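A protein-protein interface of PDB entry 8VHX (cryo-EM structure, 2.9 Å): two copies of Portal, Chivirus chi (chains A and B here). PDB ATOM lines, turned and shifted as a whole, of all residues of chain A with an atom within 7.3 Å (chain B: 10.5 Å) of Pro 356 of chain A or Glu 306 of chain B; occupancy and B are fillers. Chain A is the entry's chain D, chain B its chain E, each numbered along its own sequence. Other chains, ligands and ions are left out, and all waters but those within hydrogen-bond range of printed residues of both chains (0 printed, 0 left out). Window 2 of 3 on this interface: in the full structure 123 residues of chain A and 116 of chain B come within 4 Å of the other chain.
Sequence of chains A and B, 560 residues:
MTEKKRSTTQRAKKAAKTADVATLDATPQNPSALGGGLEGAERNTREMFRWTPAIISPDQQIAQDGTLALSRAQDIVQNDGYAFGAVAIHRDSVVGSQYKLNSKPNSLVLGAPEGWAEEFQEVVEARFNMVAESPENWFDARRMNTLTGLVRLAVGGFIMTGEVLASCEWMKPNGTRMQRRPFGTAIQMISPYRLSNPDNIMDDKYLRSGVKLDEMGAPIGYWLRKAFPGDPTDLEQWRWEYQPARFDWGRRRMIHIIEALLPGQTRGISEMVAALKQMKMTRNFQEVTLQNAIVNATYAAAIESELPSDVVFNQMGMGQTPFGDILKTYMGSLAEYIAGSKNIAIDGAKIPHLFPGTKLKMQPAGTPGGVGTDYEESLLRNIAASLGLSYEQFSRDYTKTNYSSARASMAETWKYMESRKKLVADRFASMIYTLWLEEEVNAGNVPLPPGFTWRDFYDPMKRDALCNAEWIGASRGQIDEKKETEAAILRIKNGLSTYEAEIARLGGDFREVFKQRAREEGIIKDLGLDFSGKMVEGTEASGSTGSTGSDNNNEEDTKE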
ATOM      1  N   GLU A 306     -34.701   4.197   1.014  1.00  0.00           N
ATOM      2  CA  GLU A 306     -35.588   3.151   0.542  1.00  0.00           C
ATOM      3  C   GLU A 306     -34.817   1.977  -0.023  1.00  0.00           C
ATOM      4  O   GLU A 306     -35.420   1.059  -0.582  1.00  0.00           O
ATOM      5  CB  GLU A 306     -36.546   3.738  -0.490  1.00  0.00           C
ATOM      6  CG  GLU A 306     -35.860   4.493  -1.615  1.00  0.00           C
ATOM      7  CD  GLU A 306     -36.840   5.260  -2.476  1.00  0.00           C
ATOM      8  OE1 GLU A 306     -38.057   5.096  -2.273  1.00  0.00           O
ATOM      9  OE2 GLU A 306     -36.390   6.059  -3.324  1.00  0.00           O
ATOM     10  N   LEU A 307     -33.499   2.003   0.105  1.00  0.00           N
ATOM     11  CA  LEU A 307     -32.685   0.850  -0.165  1.00  0.00           C
ATOM     12  C   LEU A 307     -32.786  -0.134   0.992  1.00  0.00           C
ATOM     13  O   LEU A 307     -33.134   0.241   2.113  1.00  0.00           O
ATOM     14  CB  LEU A 307     -31.234   1.264  -0.359  1.00  0.00           C
ATOM     15  CG  LEU A 307     -30.762   1.701  -1.738  1.00  0.00           C
ATOM     16  CD1 LEU A 307     -30.869   0.577  -2.678  1.00  0.00           C
ATOM     17  CD2 LEU A 307     -31.549   2.837  -2.268  1.00  0.00           C
ATOM     18  N   HIS A 353     -20.160   5.415  -2.166  1.00  0.00           N
ATOM     19  CA  HIS A 353     -21.030   5.822  -3.248  1.00  0.00           C
ATOM     20  C   HIS A 353     -22.452   5.471  -2.865  1.00  0.00           C
ATOM     21  O   HIS A 353     -22.762   4.305  -2.611  1.00  0.00           O
ATOM     22  CB  HIS A 353     -20.647   5.140  -4.555  1.00  0.00           C
ATOM     23  CG  HIS A 353     -21.780   4.996  -5.514  1.00  0.00           C
ATOM     24  ND1 HIS A 353     -22.162   6.005  -6.362  1.00  0.00           N
ATOM     25  CD2 HIS A 353     -22.612   3.959  -5.763  1.00  0.00           C
ATOM     26  CE1 HIS A 353     -23.183   5.602  -7.092  1.00  0.00           C
ATOM     27  NE2 HIS A 353     -23.477   4.364  -6.749  1.00  0.00           N
ATOM     28  N   LEU A 354     -23.306   6.475  -2.826  1.00  0.00           N
ATOM     29  CA  LEU A 354     -24.672   6.324  -2.379  1.00  0.00           C
ATOM     30  C   LEU A 354     -25.608   6.709  -3.505  1.00  0.00           C
ATOM     31  O   LEU A 354     -25.368   7.685  -4.215  1.00  0.00           O
ATOM     32  CB  LEU A 354     -24.929   7.189  -1.167  1.00  0.00           C
ATOM     33  CG  LEU A 354     -23.946   7.030  -0.017  1.00  0.00           C
ATOM     34  CD1 LEU A 354     -24.147   8.142   0.945  1.00  0.00           C
ATOM     35  CD2 LEU A 354     -24.117   5.726   0.684  1.00  0.00           C
ATOM     36  N   PHE A 355     -26.659   5.929  -3.681  1.00  0.00           N
ATOM     37  CA  PHE A 355     -27.629   6.238  -4.706  1.00  0.00           C
ATOM     38  C   PHE A 355     -28.474   7.432  -4.277  1.00  0.00           C
ATOM     39  O   PHE A 355     -28.671   7.670  -3.084  1.00  0.00           O
ATOM     40  CB  PHE A 355     -28.515   5.034  -4.979  1.00  0.00           C
ATOM     41  CG  PHE A 355     -27.772   3.837  -5.465  1.00  0.00           C
ATOM     42  CD1 PHE A 355     -26.878   3.937  -6.502  1.00  0.00           C
ATOM     43  CD2 PHE A 355     -27.971   2.606  -4.889  1.00  0.00           C
ATOM     44  CE1 PHE A 355     -26.207   2.846  -6.945  1.00  0.00           C
ATOM     45  CE2 PHE A 355     -27.295   1.517  -5.333  1.00  0.00           C
ATOM     46  CZ  PHE A 355     -26.415   1.633  -6.359  1.00  0.00           C
ATOM     47  N   PRO A 356     -28.979   8.206  -5.228  1.00  0.00           N
ATOM     48  CA  PRO A 356     -29.754   9.391  -4.869  1.00  0.00           C
ATOM     49  C   PRO A 356     -31.033   9.028  -4.133  1.00  0.00           C
ATOM     50  O   PRO A 356     -31.725   8.070  -4.479  1.00  0.00           O
ATOM     51  CB  PRO A 356     -30.037  10.043  -6.222  1.00  0.00           C
ATOM     52  CG  PRO A 356     -29.910   8.972  -7.180  1.00  0.00           C
ATOM     53  CD  PRO A 356     -28.858   8.073  -6.681  1.00  0.00           C
ATOM     54  N   GLY A 357     -31.347   9.824  -3.116  1.00  0.00           N
ATOM     55  CA  GLY A 357     -32.394   9.526  -2.175  1.00  0.00           C
ATOM     56  C   GLY A 357     -31.895   8.925  -0.883  1.00  0.00           C
ATOM     57  O   GLY A 357     -32.647   8.866   0.095  1.00  0.00           O
ATOM     58  N   THR A 358     -30.653   8.460  -0.870  1.00  0.00           N
ATOM     59  CA  THR A 358     -29.977   7.987   0.328  1.00  0.00           C
ATOM     60  C   THR A 358     -29.203   9.145   0.935  1.00  0.00           C
ATOM     61  O   THR A 358     -28.099   9.465   0.497  1.00  0.00           O
ATOM     62  CB  THR A 358     -29.062   6.826  -0.028  1.00  0.00           C
ATOM     63  OG1 THR A 358     -29.834   5.772  -0.607  1.00  0.00           O
ATOM     64  CG2 THR A 358     -28.340   6.304   1.170  1.00  0.00           C
ATOM     65  N   LYS A 359     -29.778   9.778   1.952  1.00  0.00           N
ATOM     66  CA  LYS A 359     -29.102  10.846   2.678  1.00  0.00           C
ATOM     67  C   LYS A 359     -28.276  10.216   3.791  1.00  0.00           C
ATOM     68  O   LYS A 359     -28.827   9.616   4.716  1.00  0.00           O
ATOM     69  CB  LYS A 359     -30.083  11.857   3.269  1.00  0.00           C
ATOM     70  CG  LYS A 359     -31.462  11.935   2.656  1.00  0.00           C
ATOM     71  CD  LYS A 359     -31.450  12.388   1.221  1.00  0.00           C
ATOM     72  CE  LYS A 359     -32.863  12.693   0.744  1.00  0.00           C
ATOM     73  NZ  LYS A 359     -33.834  11.621   1.105  1.00  0.00           N
ATOM     74  N   ALA B 302     -18.616  11.588   0.598  1.00  0.00           N
ATOM     75  CA  ALA B 302     -19.638  10.713   0.069  1.00  0.00           C
ATOM     76  C   ALA B 302     -20.137  11.256  -1.254  1.00  0.00           C
ATOM     77  O   ALA B 302     -20.341  12.459  -1.412  1.00  0.00           O
ATOM     78  CB  ALA B 302     -20.795  10.556   1.031  1.00  0.00           C
ATOM     79  N   ILE B 303     -20.342  10.351  -2.196  1.00  0.00           N
ATOM     80  CA  ILE B 303     -20.923  10.681  -3.481  1.00  0.00           C
ATOM     81  C   ILE B 303     -22.367  10.226  -3.483  1.00  0.00           C
ATOM     82  O   ILE B 303     -22.678   9.115  -3.043  1.00  0.00           O
ATOM     83  CB  ILE B 303     -20.155  10.036  -4.641  1.00  0.00           C
ATOM     84  CG1 ILE B 303     -18.734  10.546  -4.701  1.00  0.00           C
ATOM     85  CG2 ILE B 303     -20.825  10.341  -5.927  1.00  0.00           C
ATOM     86  CD1 ILE B 303     -17.793   9.650  -4.085  1.00  0.00           C
ATOM     87  N   GLU B 304     -23.246  11.085  -3.962  1.00  0.00           N
ATOM     88  CA  GLU B 304     -24.617  10.717  -4.247  1.00  0.00           C
ATOM     89  C   GLU B 304     -24.755  10.691  -5.758  1.00  0.00           C
ATOM     90  O   GLU B 304     -24.910  11.739  -6.388  1.00  0.00           O
ATOM     91  CB  GLU B 304     -25.592  11.703  -3.616  1.00  0.00           C
ATOM     92  CG  GLU B 304     -27.026  11.258  -3.607  1.00  0.00           C
ATOM     93  CD  GLU B 304     -27.952  12.279  -2.967  1.00  0.00           C
ATOM     94  OE1 GLU B 304     -27.607  13.478  -2.959  1.00  0.00           O
ATOM     95  OE2 GLU B 304     -29.024  11.882  -2.465  1.00  0.00           O
ATOM     96  N   SER B 305     -24.709   9.497  -6.332  1.00  0.00           N
ATOM     97  CA  SER B 305     -24.694   9.375  -7.775  1.00  0.00           C
ATOM     98  C   SER B 305     -25.611   8.253  -8.205  1.00  0.00           C
ATOM     99  O   SER B 305     -25.786   7.258  -7.502  1.00  0.00           O
ATOM    100  CB  SER B 305     -23.292   9.109  -8.298  1.00  0.00           C
ATOM    101  OG  SER B 305     -23.292   9.082  -9.705  1.00  0.00           O
ATOM    102  N   GLU B 306     -26.195   8.445  -9.372  1.00  0.00           N
ATOM    103  CA  GLU B 306     -26.941   7.417 -10.068  1.00  0.00           C
ATOM    104  C   GLU B 306     -26.071   6.684 -11.068  1.00  0.00           C
ATOM    105  O   GLU B 306     -26.561   5.808 -11.783  1.00  0.00           O
ATOM    106  CB  GLU B 306     -28.156   8.041 -10.753  1.00  0.00           C
ATOM    107  CG  GLU B 306     -27.835   9.216 -11.639  1.00  0.00           C
ATOM    108  CD  GLU B 306     -29.078   9.912 -12.146  1.00  0.00           C
ATOM    109  OE1 GLU B 306     -30.191   9.433 -11.851  1.00  0.00           O
ATOM    110  OE2 GLU B 306     -28.940  10.958 -12.816  1.00  0.00           O
ATOM    111  N   LEU B 307     -24.795   7.035 -11.131  1.00  0.00           N
ATOM    112  CA  LEU B 307     -23.834   6.289 -11.900  1.00  0.00           C
ATOM    113  C   LEU B 307     -23.438   5.028 -11.149  1.00  0.00           C
ATOM    114  O   LEU B 307     -23.739   4.876  -9.964  1.00  0.00           O
ATOM    115  CB  LEU B 307     -22.599   7.133 -12.158  1.00  0.00           C
ATOM    116  CG  LEU B 307     -22.849   8.451 -12.854  1.00  0.00           C
ATOM    117  CD1 LEU B 307     -21.638   9.311 -12.784  1.00  0.00           C
ATOM    118  CD2 LEU B 307     -23.200   8.187 -14.263  1.00  0.00           C
ATOM    119  N   PRO B 308     -22.775   4.099 -11.820  1.00  0.00           N
ATOM    120  CA  PRO B 308     -22.196   2.967 -11.109  1.00  0.00           C
ATOM    121  C   PRO B 308     -20.948   3.365 -10.345  1.00  0.00           C
ATOM    122  O   PRO B 308     -20.288   4.358 -10.649  1.00  0.00           O
ATOM    123  CB  PRO B 308     -21.882   1.980 -12.231  1.00  0.00           C
ATOM    124  CG  PRO B 308     -21.709   2.786 -13.389  1.00  0.00           C
ATOM    125  CD  PRO B 308     -22.595   3.961 -13.268  1.00  0.00           C
ATOM    126  N   SER B 309     -20.642   2.570  -9.325  1.00  0.00           N
ATOM    127  CA  SER B 309     -19.499   2.854  -8.472  1.00  0.00           C
ATOM    128  C   SER B 309     -18.196   2.856  -9.256  1.00  0.00           C
ATOM    129  O   SER B 309     -17.268   3.607  -8.937  1.00  0.00           O
ATOM    130  CB  SER B 309     -19.446   1.826  -7.356  1.00  0.00           C
ATOM    131  OG  SER B 309     -19.471   0.515  -7.890  1.00  0.00           O
ATOM    132  N   ASP B 310     -18.097   2.009 -10.274  1.00  0.00           N
ATOM    133  CA  ASP B 310     -16.849   1.884 -11.010  1.00  0.00           C
ATOM    134  C   ASP B 310     -16.530   3.148 -11.791  1.00  0.00           C
ATOM    135  O   ASP B 310     -15.358   3.499 -11.956  1.00  0.00           O
ATOM    136  CB  ASP B 310     -16.932   0.688 -11.949  1.00  0.00           C
ATOM    137  CG  ASP B 310     -17.131  -0.618 -11.207  1.00  0.00           C
ATOM    138  OD1 ASP B 310     -16.169  -1.100 -10.575  1.00  0.00           O
ATOM    139  OD2 ASP B 310     -18.256  -1.161 -11.248  1.00  0.00           O
ATOM    140  N   VAL B 311     -17.560   3.826 -12.289  1.00  0.00           N
ATOM    141  CA  VAL B 311     -17.376   5.095 -12.983  1.00  0.00           C
ATOM    142  C   VAL B 311     -17.016   6.191 -11.995  1.00  0.00           C
ATOM    143  O   VAL B 311     -16.069   6.958 -12.201  1.00  0.00           O
ATOM    144  CB  VAL B 311     -18.652   5.455 -13.753  1.00  0.00           C
ATOM    145  CG1 VAL B 311     -18.574   6.842 -14.251  1.00  0.00           C
ATOM    146  CG2 VAL B 311     -18.872   4.510 -14.870  1.00  0.00           C
ATOM    147  N   VAL B 312     -17.781   6.286 -10.912  1.00  0.00           N
ATOM    148  CA  VAL B 312     -17.620   7.373  -9.957  1.00  0.00           C
ATOM    149  C   VAL B 312     -16.215   7.377  -9.382  1.00  0.00           C
ATOM    150  O   VAL B 312     -15.563   8.420  -9.297  1.00  0.00           O
ATOM    151  CB  VAL B 312     -18.678   7.258  -8.855  1.00  0.00           C
ATOM    152  CG1 VAL B 312     -18.305   8.092  -7.698  1.00  0.00           C
ATOM    153  CG2 VAL B 312     -19.987   7.680  -9.384  1.00  0.00           C
ATOM    154  N   GLN B 315     -13.598   8.456 -11.777  1.00  0.00           N
ATOM    155  CA  GLN B 315     -13.540   9.910 -11.838  1.00  0.00           C
ATOM    156  C   GLN B 315     -12.699  10.481 -10.716  1.00  0.00           C
ATOM    157  O   GLN B 315     -12.058  11.521 -10.885  1.00  0.00           O
ATOM    158  CB  GLN B 315     -14.941  10.492 -11.755  1.00  0.00           C
ATOM    159  CG  GLN B 315     -15.801  10.244 -12.939  1.00  0.00           C
ATOM    160  CD  GLN B 315     -17.226  10.626 -12.694  1.00  0.00           C
ATOM    161  OE1 GLN B 315     -17.643  10.831 -11.562  1.00  0.00           O
ATOM    162  NE2 GLN B 315     -17.989  10.713 -13.752  1.00  0.00           N
ATOM    163  N   LEU B 354     -17.139  15.626 -12.416  1.00  0.00           N
ATOM    164  CA  LEU B 354     -18.306  14.877 -11.990  1.00  0.00           C
ATOM    165  C   LEU B 354     -19.501  15.300 -12.825  1.00  0.00           C
ATOM    166  O   LEU B 354     -19.779  16.494 -12.955  1.00  0.00           O
ATOM    167  CB  LEU B 354     -18.576  15.124 -10.517  1.00  0.00           C
ATOM    168  CG  LEU B 354     -17.412  14.850  -9.575  1.00  0.00           C
ATOM    169  CD1 LEU B 354     -17.682  15.527  -8.284  1.00  0.00           C
ATOM    170  CD2 LEU B 354     -17.210  13.377  -9.347  1.00  0.00           C
ATOM    171  N   PHE B 355     -20.203  14.325 -13.380  1.00  0.00           N
ATOM    172  CA  PHE B 355     -21.373  14.625 -14.178  1.00  0.00           C
ATOM    173  C   PHE B 355     -22.464  15.225 -13.295  1.00  0.00           C
ATOM    174  O   PHE B 355     -22.555  14.912 -12.107  1.00  0.00           O
ATOM    175  CB  PHE B 355     -21.887  13.367 -14.866  1.00  0.00           C
ATOM    176  CG  PHE B 355     -20.950  12.805 -15.880  1.00  0.00           C
ATOM    177  CD1 PHE B 355     -20.498  13.569 -16.932  1.00  0.00           C
ATOM    178  CD2 PHE B 355     -20.517  11.510 -15.778  1.00  0.00           C
ATOM    179  CE1 PHE B 355     -19.643  13.046 -17.851  1.00  0.00           C
ATOM    180  CE2 PHE B 355     -19.659  10.986 -16.695  1.00  0.00           C
ATOM    181  CZ  PHE B 355     -19.222  11.749 -17.731  1.00  0.00           C
ATOM    182  N   PRO B 356     -23.307  16.087 -13.851  1.00  0.00           N
ATOM    183  CA  PRO B 356     -24.351  16.711 -13.041  1.00  0.00           C
ATOM    184  C   PRO B 356     -25.316  15.674 -12.497  1.00  0.00           C
ATOM    185  O   PRO B 356     -25.675  14.711 -13.177  1.00  0.00           O
ATOM    186  CB  PRO B 356     -25.028  17.670 -14.022  1.00  0.00           C
ATOM    187  CG  PRO B 356     -24.750  17.122 -15.319  1.00  0.00           C
ATOM    188  CD  PRO B 356     -23.404  16.501 -15.252  1.00  0.00           C
ATOM    189  N   GLY B 357     -25.732  15.877 -11.255  1.00  0.00           N
ATOM    190  CA  GLY B 357     -26.453  14.872 -10.518  1.00  0.00           C
ATOM    191  C   GLY B 357     -25.573  13.979  -9.686  1.00  0.00           C
ATOM    192  O   GLY B 357     -26.088  13.219  -8.857  1.00  0.00           O
ATOM    193  N   THR B 358     -24.266  14.029  -9.901  1.00  0.00           N
ATOM    194  CA  THR B 358     -23.300  13.426  -9.002  1.00  0.00           C
ATOM    195  C   THR B 358     -22.803  14.500  -8.050  1.00  0.00           C
ATOM    196  O   THR B 358     -22.175  15.473  -8.478  1.00  0.00           O
ATOM    197  CB  THR B 358     -22.144  12.815  -9.782  1.00  0.00           C
ATOM    198  OG1 THR B 358     -22.634  11.780 -10.633  1.00  0.00           O
ATOM    199  CG2 THR B 358     -21.138  12.238  -8.849  1.00  0.00           C
ATOM    200  N   LYS B 359     -23.089  14.327  -6.770  1.00  0.00           N
ATOM    201  CA  LYS B 359     -22.737  15.293  -5.744  1.00  0.00           C
ATOM    202  C   LYS B 359     -21.617  14.714  -4.903  1.00  0.00           C
ATOM    203  O   LYS B 359     -21.755  13.622  -4.351  1.00  0.00           O
ATOM    204  CB  LYS B 359     -23.938  15.628  -4.869  1.00  0.00           C
ATOM    205  CG  LYS B 359     -25.195  15.924  -5.634  1.00  0.00           C
ATOM    206  CD  LYS B 359     -26.348  16.164  -4.701  1.00  0.00           C
ATOM    207  CE  LYS B 359     -27.670  16.041  -5.420  1.00  0.00           C
ATOM    208  NZ  LYS B 359     -28.818  15.929  -4.479  1.00  0.00           N
ATOM    209  N   LEU B 360     -20.517  15.440  -4.816  1.00  0.00           N
ATOM    210  CA  LEU B 360     -19.411  15.083  -3.947  1.00  0.00           C
ATOM    211  C   LEU B 360     -19.508  15.944  -2.701  1.00  0.00           C
ATOM    212  O   LEU B 360     -19.264  17.152  -2.755  1.00  0.00           O
ATOM    213  CB  LEU B 360     -18.079  15.291  -4.652  1.00  0.00           C
ATOM    214  CG  LEU B 360     -16.843  15.084  -3.802  1.00  0.00           C
ATOM    215  CD1 LEU B 360     -16.744  13.634  -3.406  1.00  0.00           C
ATOM    216  CD2 LEU B 360     -15.629  15.519  -4.554  1.00  0.00           C
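O of Leu 307 of chain B sits close to NE2 of His 353 of chain A (3.3 Å).
N of Leu 354 of chain A sits at hydrogen-bond distance from O of Ile 303 of chain B.
N of Ser 305 of chain B sits at hydrogen-bond distance from O of Leu 354 of chain A.
The side-chain carboxylate (OE2) of Glu 304 of chain B sits at hydrogen-bond distance from the backbone NH (N) of Gly 357 of chain A (3.2 Å).
OG1 of Thr 358 of chain A lies close to O of Phe 355 of chain A (3.3 Å).
O of Gly 357 of chain A lies within hydrogen-bond range of NZ of Lys 359 of chain A (3.2 Å).
OE1 of Glu 304 of chain B lies within salt-bridge range of NZ of Lys 359 of chain B (3.1 Å).
The backbone NH of Leu 307 of chain B lies within hydrogen-bond range of the side-chain hydroxyl of Ser 305 of chain B (2.9 Å).
The side-chain hydroxyl of Thr 358 of chain B sits at hydrogen-bond distance from the side-chain hydroxyl of Ser 305 of chain B (2.9 Å).
His 353 of chain A touches Ile 303 of chain B.
Ser 305 of chain B touches His 353 of chain A.
Leu 354 of chain A touches Glu 304 of chain B (O to CA, 3.1 Å).
O of Phe 355 of chain A touches CG of Glu 304 of chain B, at 3.98 Å.
CA of Phe 355 of chain A touches O of Ser 305 of chain B, at 3.5 Å.
Glu 304 of chain B touches Pro 356 of chain A (OE2 to CA, 3.5 Å).
Ser 305 of chain B touches Pro 356 of chain A.
Pro 356 of chain A touches Glu 306 of chain B.
OE2 of Glu 304 of chain B touches O of Thr 358 of chain A, at 3.9 Å.
Pro 356 of chain A touches just these residues of chain B: Glu 304, Ser 305 and Glu 306.
Glu 306 of chain B touches just one residue of chain A: Pro 356 (3.8 Å).
Gly 357 of chain A touches just one residue of chain B: Glu 304 (3.2 Å).
Printed residues of chain B within 4 Å of Leu 354 of chain A: Ile 303, Glu 304 and Ser 305.
Of the printed residues of chain A, Leu 307 of chain B touches His 353.
Of the printed residues of chain B, Phe 355 of chain A touches Glu 304 and Ser 305.
Of the printed residues of chain A, Ser 305 of chain B touches His 353, Leu 354, Phe 355 and Pro 356.
Gly 357 of chain B touches none of the printed residues of chain A.
The nearest residue of chain B that does not touch Pro 356 of chain A is Gly 357 of chain B (5.7 Å).
The nearest printed residue of chain A that does not touch Leu 307 of chain B is Phe 355 of chain A (4.4 Å).
Of the 19 printed residues of chain B, 5 touch a printed residue of chain A.
Printed residues of chain B that touch a printed residue of chain A: Ile 303, Glu 304, Ser 305, Glu 306 and Leu 307.
Among the printed residues, no Asp or Glu carboxylate lies within 4 Å of a Lys or Arg side-chain nitrogen of the other chain.
Pro 356 of chain A touches Glu 306 of chain B, but with the chains exchanged Glu 306 of chain A does not touch Pro 356 of chain B (16.9 Å).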
